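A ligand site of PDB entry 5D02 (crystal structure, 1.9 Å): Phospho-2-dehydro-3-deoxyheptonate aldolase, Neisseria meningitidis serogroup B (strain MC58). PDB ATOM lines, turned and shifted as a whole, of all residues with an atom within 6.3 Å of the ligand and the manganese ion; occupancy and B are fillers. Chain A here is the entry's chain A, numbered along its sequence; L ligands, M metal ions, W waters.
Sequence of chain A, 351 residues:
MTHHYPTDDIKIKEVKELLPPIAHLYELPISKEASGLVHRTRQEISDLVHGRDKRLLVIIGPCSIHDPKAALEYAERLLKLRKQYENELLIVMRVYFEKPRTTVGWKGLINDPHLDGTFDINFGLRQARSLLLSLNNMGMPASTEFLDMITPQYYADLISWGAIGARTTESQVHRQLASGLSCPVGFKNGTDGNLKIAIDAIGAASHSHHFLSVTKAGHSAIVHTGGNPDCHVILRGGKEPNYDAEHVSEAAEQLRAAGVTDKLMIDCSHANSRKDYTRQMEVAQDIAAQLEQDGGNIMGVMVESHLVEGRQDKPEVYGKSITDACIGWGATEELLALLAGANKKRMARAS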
ATOM      1  N   CYS A  63     -18.937   3.135   1.732  1.00  0.00           N
ATOM      2  CA  CYS A  63     -19.080   2.233   2.835  1.00  0.00           C
ATOM      3  C   CYS A  63     -20.460   1.569   2.755  1.00  0.00           C
ATOM      4  O   CYS A  63     -20.595   0.344   2.843  1.00  0.00           O
ATOM      5  CB  CYS A  63     -18.931   2.983   4.172  1.00  0.00           C
ATOM      6  SG  CYS A  63     -19.277   1.903   5.618  1.00  0.00           S
ATOM      7  N   SER A  64     -21.489   2.400   2.561  1.00  0.00           N
ATOM      8  CA  SER A  64     -22.863   1.958   2.407  1.00  0.00           C
ATOM      9  C   SER A  64     -23.639   2.795   1.351  1.00  0.00           C
ATOM     10  O   SER A  64     -23.361   3.984   1.173  1.00  0.00           O
ATOM     11  CB  SER A  64     -23.598   2.051   3.730  1.00  0.00           C
ATOM     12  OG  SER A  64     -23.693   3.377   4.216  1.00  0.00           O
ATOM     13  N   ARG A  94     -18.278  -1.065  -5.053  1.00  0.00           N
ATOM     14  CA  ARG A  94     -18.856  -1.430  -3.761  1.00  0.00           C
ATOM     15  C   ARG A  94     -20.292  -0.947  -3.733  1.00  0.00           C
ATOM     16  O   ARG A  94     -20.538   0.281  -3.782  1.00  0.00           O
ATOM     17  CB  ARG A  94     -18.150  -0.681  -2.604  1.00  0.00           C
ATOM     18  CG  ARG A  94     -16.980  -1.358  -1.996  1.00  0.00           C
ATOM     19  CD  ARG A  94     -16.441  -0.636  -0.744  1.00  0.00           C
ATOM     20  NE  ARG A  94     -17.337  -0.585   0.408  1.00  0.00           N
ATOM     21  CZ  ARG A  94     -17.216  -1.318   1.525  1.00  0.00           C
ATOM     22  NH1 ARG A  94     -16.203  -2.167   1.699  1.00  0.00           N
ATOM     23  NH2 ARG A  94     -18.099  -1.185   2.505  1.00  0.00           N
ATOM     24  N   TYR A  96     -22.909  -1.814  -1.116  1.00  0.00           N
ATOM     25  CA  TYR A  96     -23.229  -2.511   0.134  1.00  0.00           C
ATOM     26  C   TYR A  96     -24.564  -2.011   0.697  1.00  0.00           C
ATOM     27  O   TYR A  96     -24.700  -0.848   1.010  1.00  0.00           O
ATOM     28  CB  TYR A  96     -22.130  -2.323   1.158  1.00  0.00           C
ATOM     29  CG  TYR A  96     -20.890  -3.200   0.951  1.00  0.00           C
ATOM     30  CD1 TYR A  96     -20.327  -3.388  -0.315  1.00  0.00           C
ATOM     31  CD2 TYR A  96     -20.265  -3.800   2.016  1.00  0.00           C
ATOM     32  CE1 TYR A  96     -19.206  -4.184  -0.489  1.00  0.00           C
ATOM     33  CE2 TYR A  96     -19.107  -4.558   1.854  1.00  0.00           C
ATOM     34  CZ  TYR A  96     -18.583  -4.742   0.597  1.00  0.00           C
ATOM     35  OH  TYR A  96     -17.469  -5.501   0.422  1.00  0.00           O
ATOM     36  N   GLU A  98     -26.235  -4.076   3.065  1.00  0.00           N
ATOM     37  CA  GLU A  98     -26.325  -4.654   4.431  1.00  0.00           C
ATOM     38  C   GLU A  98     -25.055  -4.392   5.256  1.00  0.00           C
ATOM     39  O   GLU A  98     -23.932  -4.741   4.842  1.00  0.00           O
ATOM     40  CB  GLU A  98     -26.590  -6.178   4.374  1.00  0.00           C
ATOM     41  CG  GLU A  98     -27.615  -6.538   3.336  1.00  0.00           C
ATOM     42  CD  GLU A  98     -28.011  -8.006   3.363  1.00  0.00           C
ATOM     43  OE1 GLU A  98     -27.117  -8.891   3.323  1.00  0.00           O
ATOM     44  OE2 GLU A  98     -29.244  -8.227   3.399  1.00  0.00           O
ATOM     45  N   LYS A  99     -25.283  -3.819   6.434  1.00  0.00           N
ATOM     46  CA  LYS A  99     -24.232  -3.311   7.333  1.00  0.00           C
ATOM     47  C   LYS A  99     -24.320  -3.968   8.696  1.00  0.00           C
ATOM     48  O   LYS A  99     -25.382  -3.937   9.349  1.00  0.00           O
ATOM     49  CB  LYS A  99     -24.358  -1.779   7.532  1.00  0.00           C
ATOM     50  CG  LYS A  99     -24.312  -1.013   6.264  1.00  0.00           C
ATOM     51  CD  LYS A  99     -23.126  -1.427   5.386  1.00  0.00           C
ATOM     52  CE  LYS A  99     -21.782  -0.911   5.961  1.00  0.00           C
ATOM     53  NZ  LYS A  99     -20.681  -1.394   5.149  1.00  0.00           N
ATOM     54  N   PRO A 100     -23.199  -4.531   9.162  1.00  0.00           N
ATOM     55  CA  PRO A 100     -23.170  -5.161  10.484  1.00  0.00           C
ATOM     56  C   PRO A 100     -22.780  -4.112  11.515  1.00  0.00           C
ATOM     57  O   PRO A 100     -21.757  -3.461  11.364  1.00  0.00           O
ATOM     58  CB  PRO A 100     -22.086  -6.222  10.349  1.00  0.00           C
ATOM     59  CG  PRO A 100     -21.194  -5.763   9.247  1.00  0.00           C
ATOM     60  CD  PRO A 100     -21.979  -4.788   8.384  1.00  0.00           C
ATOM     61  N   GLU A 145     -21.635  -7.061   0.499  1.00  0.00           N
ATOM     62  CA  GLU A 145     -21.433  -8.002   1.603  1.00  0.00           C
ATOM     63  C   GLU A 145     -22.753  -8.731   1.794  1.00  0.00           C
ATOM     64  O   GLU A 145     -23.799  -8.085   1.949  1.00  0.00           O
ATOM     65  CB  GLU A 145     -21.046  -7.337   2.941  1.00  0.00           C
ATOM     66  CG  GLU A 145     -20.911  -8.363   4.105  1.00  0.00           C
ATOM     67  CD  GLU A 145     -20.719  -7.792   5.534  1.00  0.00           C
ATOM     68  OE1 GLU A 145     -20.215  -6.671   5.689  1.00  0.00           O
ATOM     69  OE2 GLU A 145     -21.082  -8.492   6.524  1.00  0.00           O
ATOM     70  N   ALA A 163     -18.595 -10.338  -0.401  1.00  0.00           N
ATOM     71  CA  ALA A 163     -17.817 -10.407   0.826  1.00  0.00           C
ATOM     72  C   ALA A 163     -18.608 -11.044   1.950  1.00  0.00           C
ATOM     73  O   ALA A 163     -19.849 -10.920   2.040  1.00  0.00           O
ATOM     74  CB  ALA A 163     -17.346  -9.009   1.241  1.00  0.00           C
ATOM     75  N   ILE A 164     -17.871 -11.748   2.807  1.00  0.00           N
ATOM     76  CA  ILE A 164     -18.356 -12.162   4.125  1.00  0.00           C
ATOM     77  C   ILE A 164     -17.558 -11.337   5.143  1.00  0.00           C
ATOM     78  O   ILE A 164     -16.301 -11.341   5.175  1.00  0.00           O
ATOM     79  CB  ILE A 164     -18.199 -13.687   4.371  1.00  0.00           C
ATOM     80  CG1 ILE A 164     -18.970 -14.513   3.333  1.00  0.00           C
ATOM     81  CG2 ILE A 164     -18.645 -14.085   5.771  1.00  0.00           C
ATOM     82  CD1 ILE A 164     -20.478 -14.345   3.306  1.00  0.00           C
ATOM     83  N   GLY A 165     -18.262 -10.586   5.971  1.00  0.00           N
ATOM     84  CA  GLY A 165     -17.587  -9.644   6.890  1.00  0.00           C
ATOM     85  C   GLY A 165     -16.786 -10.288   7.981  1.00  0.00           C
ATOM     86  O   GLY A 165     -16.922 -11.472   8.298  1.00  0.00           O
ATOM     87  N   ALA A 166     -15.969  -9.488   8.607  1.00  0.00           N
ATOM     88  CA  ALA A 166     -15.156  -9.897   9.704  1.00  0.00           C
ATOM     89  C   ALA A 166     -15.945 -10.529  10.836  1.00  0.00           C
ATOM     90  O   ALA A 166     -15.440 -11.462  11.468  1.00  0.00           O
ATOM     91  CB  ALA A 166     -14.368  -8.710  10.212  1.00  0.00           C
ATOM     92  N   ARG A 167     -17.161 -10.029  11.078  1.00  0.00           N
ATOM     93  CA  ARG A 167     -17.976 -10.478  12.201  1.00  0.00           C
ATOM     94  C   ARG A 167     -18.720 -11.794  11.916  1.00  0.00           C
ATOM     95  O   ARG A 167     -19.388 -12.334  12.796  1.00  0.00           O
ATOM     96  CB  ARG A 167     -18.987  -9.387  12.581  1.00  0.00           C
ATOM     97  CG  ARG A 167     -18.262  -8.159  13.113  1.00  0.00           C
ATOM     98  CD  ARG A 167     -19.141  -6.944  13.330  1.00  0.00           C
ATOM     99  NE  ARG A 167     -18.299  -5.767  13.608  1.00  0.00           N
ATOM    100  CZ  ARG A 167     -17.601  -5.056  12.700  1.00  0.00           C
ATOM    101  NH1 ARG A 167     -17.570  -5.365  11.391  1.00  0.00           N
ATOM    102  NH2 ARG A 167     -16.888  -4.014  13.109  1.00  0.00           N
ATOM    103  N   LYS A 188     -13.185 -11.843   5.153  1.00  0.00           N
ATOM    104  CA  LYS A 188     -12.350 -10.946   5.919  1.00  0.00           C
ATOM    105  C   LYS A 188     -11.780 -11.621   7.152  1.00  0.00           C
ATOM    106  O   LYS A 188     -12.457 -12.407   7.800  1.00  0.00           O
ATOM    107  CB  LYS A 188     -13.171  -9.744   6.327  1.00  0.00           C
ATOM    108  CG  LYS A 188     -13.448  -8.855   5.129  1.00  0.00           C
ATOM    109  CD  LYS A 188     -13.974  -7.504   5.506  1.00  0.00           C
ATOM    110  CE  LYS A 188     -13.325  -6.459   4.606  1.00  0.00           C
ATOM    111  NZ  LYS A 188     -13.713  -5.124   5.114  1.00  0.00           N
ATOM    112  N   ASN A 189     -10.567 -11.243   7.547  1.00  0.00           N
ATOM    113  CA  ASN A 189     -10.049 -11.724   8.837  1.00  0.00           C
ATOM    114  C   ASN A 189     -10.852 -11.134  10.004  1.00  0.00           C
ATOM    115  O   ASN A 189     -11.597 -10.181   9.842  1.00  0.00           O
ATOM    116  CB  ASN A 189      -8.554 -11.424   8.992  1.00  0.00           C
ATOM    117  CG  ASN A 189      -8.250  -9.940   9.109  1.00  0.00           C
ATOM    118  OD1 ASN A 189      -7.678  -9.349   8.188  1.00  0.00           O
ATOM    119  ND2 ASN A 189      -8.610  -9.323  10.223  1.00  0.00           N
ATOM    120  N   THR A 191     -12.145  -9.437  13.673  1.00  0.00           N
ATOM    121  CA  THR A 191     -12.083  -8.036  14.095  1.00  0.00           C
ATOM    122  C   THR A 191     -10.827  -7.708  14.924  1.00  0.00           C
ATOM    123  O   THR A 191     -10.378  -6.592  14.915  1.00  0.00           O
ATOM    124  CB  THR A 191     -13.370  -7.587  14.815  1.00  0.00           C
ATOM    125  OG1 THR A 191     -13.655  -8.482  15.874  1.00  0.00           O
ATOM    126  CG2 THR A 191     -14.527  -7.644  13.900  1.00  0.00           C
ATOM    127  N   ARG A 236      -7.860  -6.939   6.572  1.00  0.00           N
ATOM    128  CA  ARG A 236      -8.543  -5.690   6.929  1.00  0.00           C
ATOM    129  C   ARG A 236      -8.160  -5.104   8.280  1.00  0.00           C
ATOM    130  O   ARG A 236      -8.859  -4.238   8.831  1.00  0.00           O
ATOM    131  CB  ARG A 236     -10.084  -5.873   6.798  1.00  0.00           C
ATOM    132  CG  ARG A 236     -10.701  -7.065   7.570  1.00  0.00           C
ATOM    133  CD  ARG A 236     -10.728  -6.820   9.073  1.00  0.00           C
ATOM    134  NE  ARG A 236     -11.755  -5.852   9.476  1.00  0.00           N
ATOM    135  CZ  ARG A 236     -11.877  -5.300  10.681  1.00  0.00           C
ATOM    136  NH1 ARG A 236     -12.875  -4.448  10.933  1.00  0.00           N
ATOM    137  NH2 ARG A 236     -10.992  -5.572  11.622  1.00  0.00           N
ATOM    138  N   ASP A 267      -7.664  -4.698   2.233  1.00  0.00           N
ATOM    139  CA  ASP A 267      -8.590  -3.587   2.467  1.00  0.00           C
ATOM    140  C   ASP A 267      -7.753  -2.420   2.977  1.00  0.00           C
ATOM    141  O   ASP A 267      -7.025  -2.561   3.936  1.00  0.00           O
ATOM    142  CB  ASP A 267      -9.671  -4.030   3.491  1.00  0.00           C
ATOM    143  CG  ASP A 267     -10.753  -2.951   3.781  1.00  0.00           C
ATOM    144  OD1 ASP A 267     -10.713  -1.814   3.214  1.00  0.00           O
ATOM    145  OD2 ASP A 267     -11.660  -3.285   4.603  1.00  0.00           O
ATOM    146  N   SER A 269      -9.130   0.298   4.136  1.00  0.00           N
ATOM    147  CA  SER A 269      -9.959   1.010   5.121  1.00  0.00           C
ATOM    148  C   SER A 269     -10.114   0.171   6.387  1.00  0.00           C
ATOM    149  O   SER A 269      -9.246  -0.669   6.699  1.00  0.00           O
ATOM    150  CB  SER A 269     -11.316   1.367   4.493  1.00  0.00           C
ATOM    151  OG  SER A 269     -12.003   2.411   5.174  1.00  0.00           O
ATOM    152  N   HIS A 270     -11.171   0.438   7.163  1.00  0.00           N
ATOM    153  CA  HIS A 270     -11.461  -0.262   8.407  1.00  0.00           C
ATOM    154  C   HIS A 270     -10.242  -0.304   9.320  1.00  0.00           C
ATOM    155  O   HIS A 270      -9.654   0.725   9.577  1.00  0.00           O
ATOM    156  CB  HIS A 270     -12.108  -1.609   8.106  1.00  0.00           C
ATOM    157  CG  HIS A 270     -13.297  -1.453   7.238  1.00  0.00           C
ATOM    158  ND1 HIS A 270     -13.283  -1.742   5.892  1.00  0.00           N
ATOM    159  CD2 HIS A 270     -14.505  -0.900   7.500  1.00  0.00           C
ATOM    160  CE1 HIS A 270     -14.436  -1.397   5.361  1.00  0.00           C
ATOM    161  NE2 HIS A 270     -15.206  -0.896   6.329  1.00  0.00           N
ATOM    162  N   ALA A 271      -9.858  -1.466   9.815  1.00  0.00           N
ATOM    163  CA  ALA A 271      -8.799  -1.497  10.790  1.00  0.00           C
ATOM    164  C   ALA A 271      -7.411  -1.364  10.204  1.00  0.00           C
ATOM    165  O   ALA A 271      -6.427  -1.285  10.967  1.00  0.00           O
ATOM    166  CB  ALA A 271      -8.885  -2.733  11.672  1.00  0.00           C
ATOM    167  N   MET A 302      -9.323  -3.167  -1.584  1.00  0.00           N
ATOM    168  CA  MET A 302     -10.652  -2.673  -1.241  1.00  0.00           C
ATOM    169  C   MET A 302     -10.482  -1.249  -0.751  1.00  0.00           C
ATOM    170  O   MET A 302      -9.518  -0.955  -0.036  1.00  0.00           O
ATOM    171  CB  MET A 302     -11.339  -3.557  -0.198  1.00  0.00           C
ATOM    172  CG  MET A 302     -12.675  -3.013   0.290  1.00  0.00           C
ATOM    173  SD  MET A 302     -13.509  -4.131   1.470  1.00  0.00           S
ATOM    174  CE  MET A 302     -14.047  -5.474   0.401  1.00  0.00           C
ATOM    175  N   GLU A 304     -12.780   2.439   0.479  1.00  0.00           N
ATOM    176  CA  GLU A 304     -14.003   3.140   0.849  1.00  0.00           C
ATOM    177  C   GLU A 304     -13.958   4.586   0.322  1.00  0.00           C
ATOM    178  O   GLU A 304     -13.210   5.434   0.837  1.00  0.00           O
ATOM    179  CB  GLU A 304     -14.224   3.056   2.355  1.00  0.00           C
ATOM    180  CG  GLU A 304     -14.737   1.689   2.766  1.00  0.00           C
ATOM    181  CD  GLU A 304     -15.282   1.637   4.178  1.00  0.00           C
ATOM    182  OE1 GLU A 304     -14.570   2.066   5.105  1.00  0.00           O
ATOM    183  OE2 GLU A 304     -16.402   1.110   4.350  1.00  0.00           O
ATOM    184  N   THR A 323     -22.194   6.215   7.098  1.00  0.00           N
ATOM    185  CA  THR A 323     -21.568   5.161   7.924  1.00  0.00           C
ATOM    186  C   THR A 323     -20.074   5.497   8.011  1.00  0.00           C
ATOM    187  O   THR A 323     -19.746   6.598   8.415  1.00  0.00           O
ATOM    188  CB  THR A 323     -21.898   3.752   7.400  1.00  0.00           C
ATOM    189  OG1 THR A 323     -21.645   3.651   5.981  1.00  0.00           O
ATOM    190  CG2 THR A 323     -23.364   3.460   7.676  1.00  0.00           C
ATOM    191  N   ASP A 324     -19.160   4.635   7.607  1.00  0.00           N
ATOM    192  CA  ASP A 324     -17.722   4.992   7.759  1.00  0.00           C
ATOM    193  C   ASP A 324     -17.310   6.133   6.809  1.00  0.00           C
ATOM    194  O   ASP A 324     -17.865   6.296   5.733  1.00  0.00           O
ATOM    195  CB  ASP A 324     -16.797   3.812   7.502  1.00  0.00           C
ATOM    196  CG  ASP A 324     -17.046   2.658   8.455  1.00  0.00           C
ATOM    197  OD1 ASP A 324     -17.417   2.866   9.599  1.00  0.00           O
ATOM    198  OD2 ASP A 324     -16.881   1.527   8.017  1.00  0.00           O
HETATM  199  C1  LIG L   1     -17.229  -3.382   5.082  1.00  0.00           C
HETATM  200  O1  LIG L   1     -16.405  -3.824   4.249  1.00  0.00           O
HETATM  201  O2  LIG L   1     -17.936  -2.360   4.972  1.00  0.00           O
HETATM  202  C2  LIG L   1     -17.249  -4.002   6.357  1.00  0.00           C
HETATM  203  C3  LIG L   1     -18.365  -4.082   7.100  1.00  0.00           C
HETATM  204  O3  LIG L   1     -15.946  -4.381   6.781  1.00  0.00           O
HETATM  205  P1  LIG L   1     -15.581  -5.333   8.084  1.00  0.00           P
HETATM  206  O4  LIG L   1     -16.412  -6.627   8.014  1.00  0.00           O
HETATM  207  O5  LIG L   1     -14.065  -5.366   7.844  1.00  0.00           O
HETATM  208  O6  LIG L   1     -15.905  -4.470   9.266  1.00  0.00           O
HETATM  209 MN    MN M   1     -17.152   0.494   6.166  1.00  0.00          MN
HETATM  210  O   HOH W   1     -15.451  -2.223  10.867  1.00  0.00           O
HETATM  211  O   HOH W   2     -21.248  -4.222   5.303  1.00  0.00           O
HETATM  212  O   HOH W   3     -17.725  -6.884   5.034  1.00  0.00           O
HETATM  213  O   HOH W   4     -16.404  -6.118   2.938  1.00  0.00           O
HETATM  214  O   HOH W   5     -18.551  -0.841   7.035  1.00  0.00           O
HETATM  215  O   HOH W   6     -18.403  -7.764   9.808  1.00  0.00           O
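The side-chain amino group of Lys 188 lies within salt-bridge range of an oxygen (O5) of the ligand (2.8 Å).
The guanidinium group (NH1) of Arg 167 is in salt-bridge range of an oxygen (O6) of the ligand (2.8 Å).
N of Ala 166 lies within hydrogen-bond range of O4 of the ligand (3.0 Å).
An oxygen (O2) of the ligand is in salt-bridge range of the side-chain amino group of Lys 99.
The guanidinium group (NE) of Arg 236 lies within salt-bridge range of an oxygen (O5) of the ligand, at 2.9 Å.
NE2 of His 270 sits close to O2 of the ligand, 3.4 Å away.
NH2 of Arg 94 is in salt-bridge range of O2 of the ligand, 2.7 Å away.
The backbone carbonyl oxygen of Ile 164 is in hydrogen-bond range of the backbone NH of Lys 188 (3.2 Å).
The side-chain amino group (NZ) of Lys 188 is in salt-bridge range of the side-chain carboxylate (OD2) of Asp 267, 2.8 Å away.
The guanidinium group (NH2) of Arg 94 sits at hydrogen-bond distance from the backbone carbonyl oxygen (O) of Cys 63.
ND1 of His 270 is in hydrogen-bond range of OD2 of Asp 267.
ND1 of His 270 lies within hydrogen-bond range of NZ of Lys 188 (3.5 Å).
NH1 of Arg 94 is in hydrogen-bond range of SD of Met 302, 3.3 Å away.
SG of Cys 63 lies close to OG1 of Thr 323, at 3.0 Å.
The side-chain carboxylate of Glu 304 lies close to the guanidinium group of Arg 94, at 3.4 Å.
Tyr 96 touches the ligand (CE2 to O1, 3.7 Å).
Pro 100 touches the ligand.
OE1 of Glu 145 touches C3 of the ligand (3.5 Å).
Gly 165 touches the ligand (CA to O4, 3.4 Å).
12 residues have an atom within 4 Å of the ligand: Arg 94, Tyr 96, Lys 99, Pro 100, Glu 145, Gly 165, Ala 166, Arg 167, Lys 188, Arg 236, His 270 and Glu 304.
The nearest printed residue that does not touch the manganese ion is Lys 99 (4.1 Å).
The side-chain carboxylate (OE2) of Glu 304 binds the manganese ion (2.1 Å).
Water W5 is bound to the manganese ion, at 2.1 Å.
The manganese ion is bound by OD2 of Asp 324.
A ring nitrogen (NE2) of His 270 is bound to the manganese ion (2.4 Å).
SG of Cys 63 is bound to the manganese ion (2.6 Å).
Water W5 bridges O2 of the ligand (2.6 Å) and NZ of Lys 99 (2.9 Å).
Water W4 bridges O1 of the ligand and OH of Tyr 96.
Water W1 lies within hydrogen-bond range of O6 of the ligand (2.8 Å), NH2 of Arg 167 (3.2 Å) and NH1 of Arg 236 (3.4 Å).
Water W6 lies within hydrogen-bond range of the backbone NH (N) of Arg 167 (2.9 Å), an oxygen (O4) of the ligand (2.9 Å) and the backbone NH (N) of Ala 166 (3.2 Å).
Water W3 bridges OE1 of Glu 145 (2.6 Å) and O4 of the ligand (3.3 Å).
Water W2 lies within hydrogen-bond range of the side-chain carboxylate of Glu 145 (2.7 Å), the backbone carbonyl oxygen of Glu 98 (2.8 Å) and the side-chain amino group of Lys 99 (2.9 Å).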
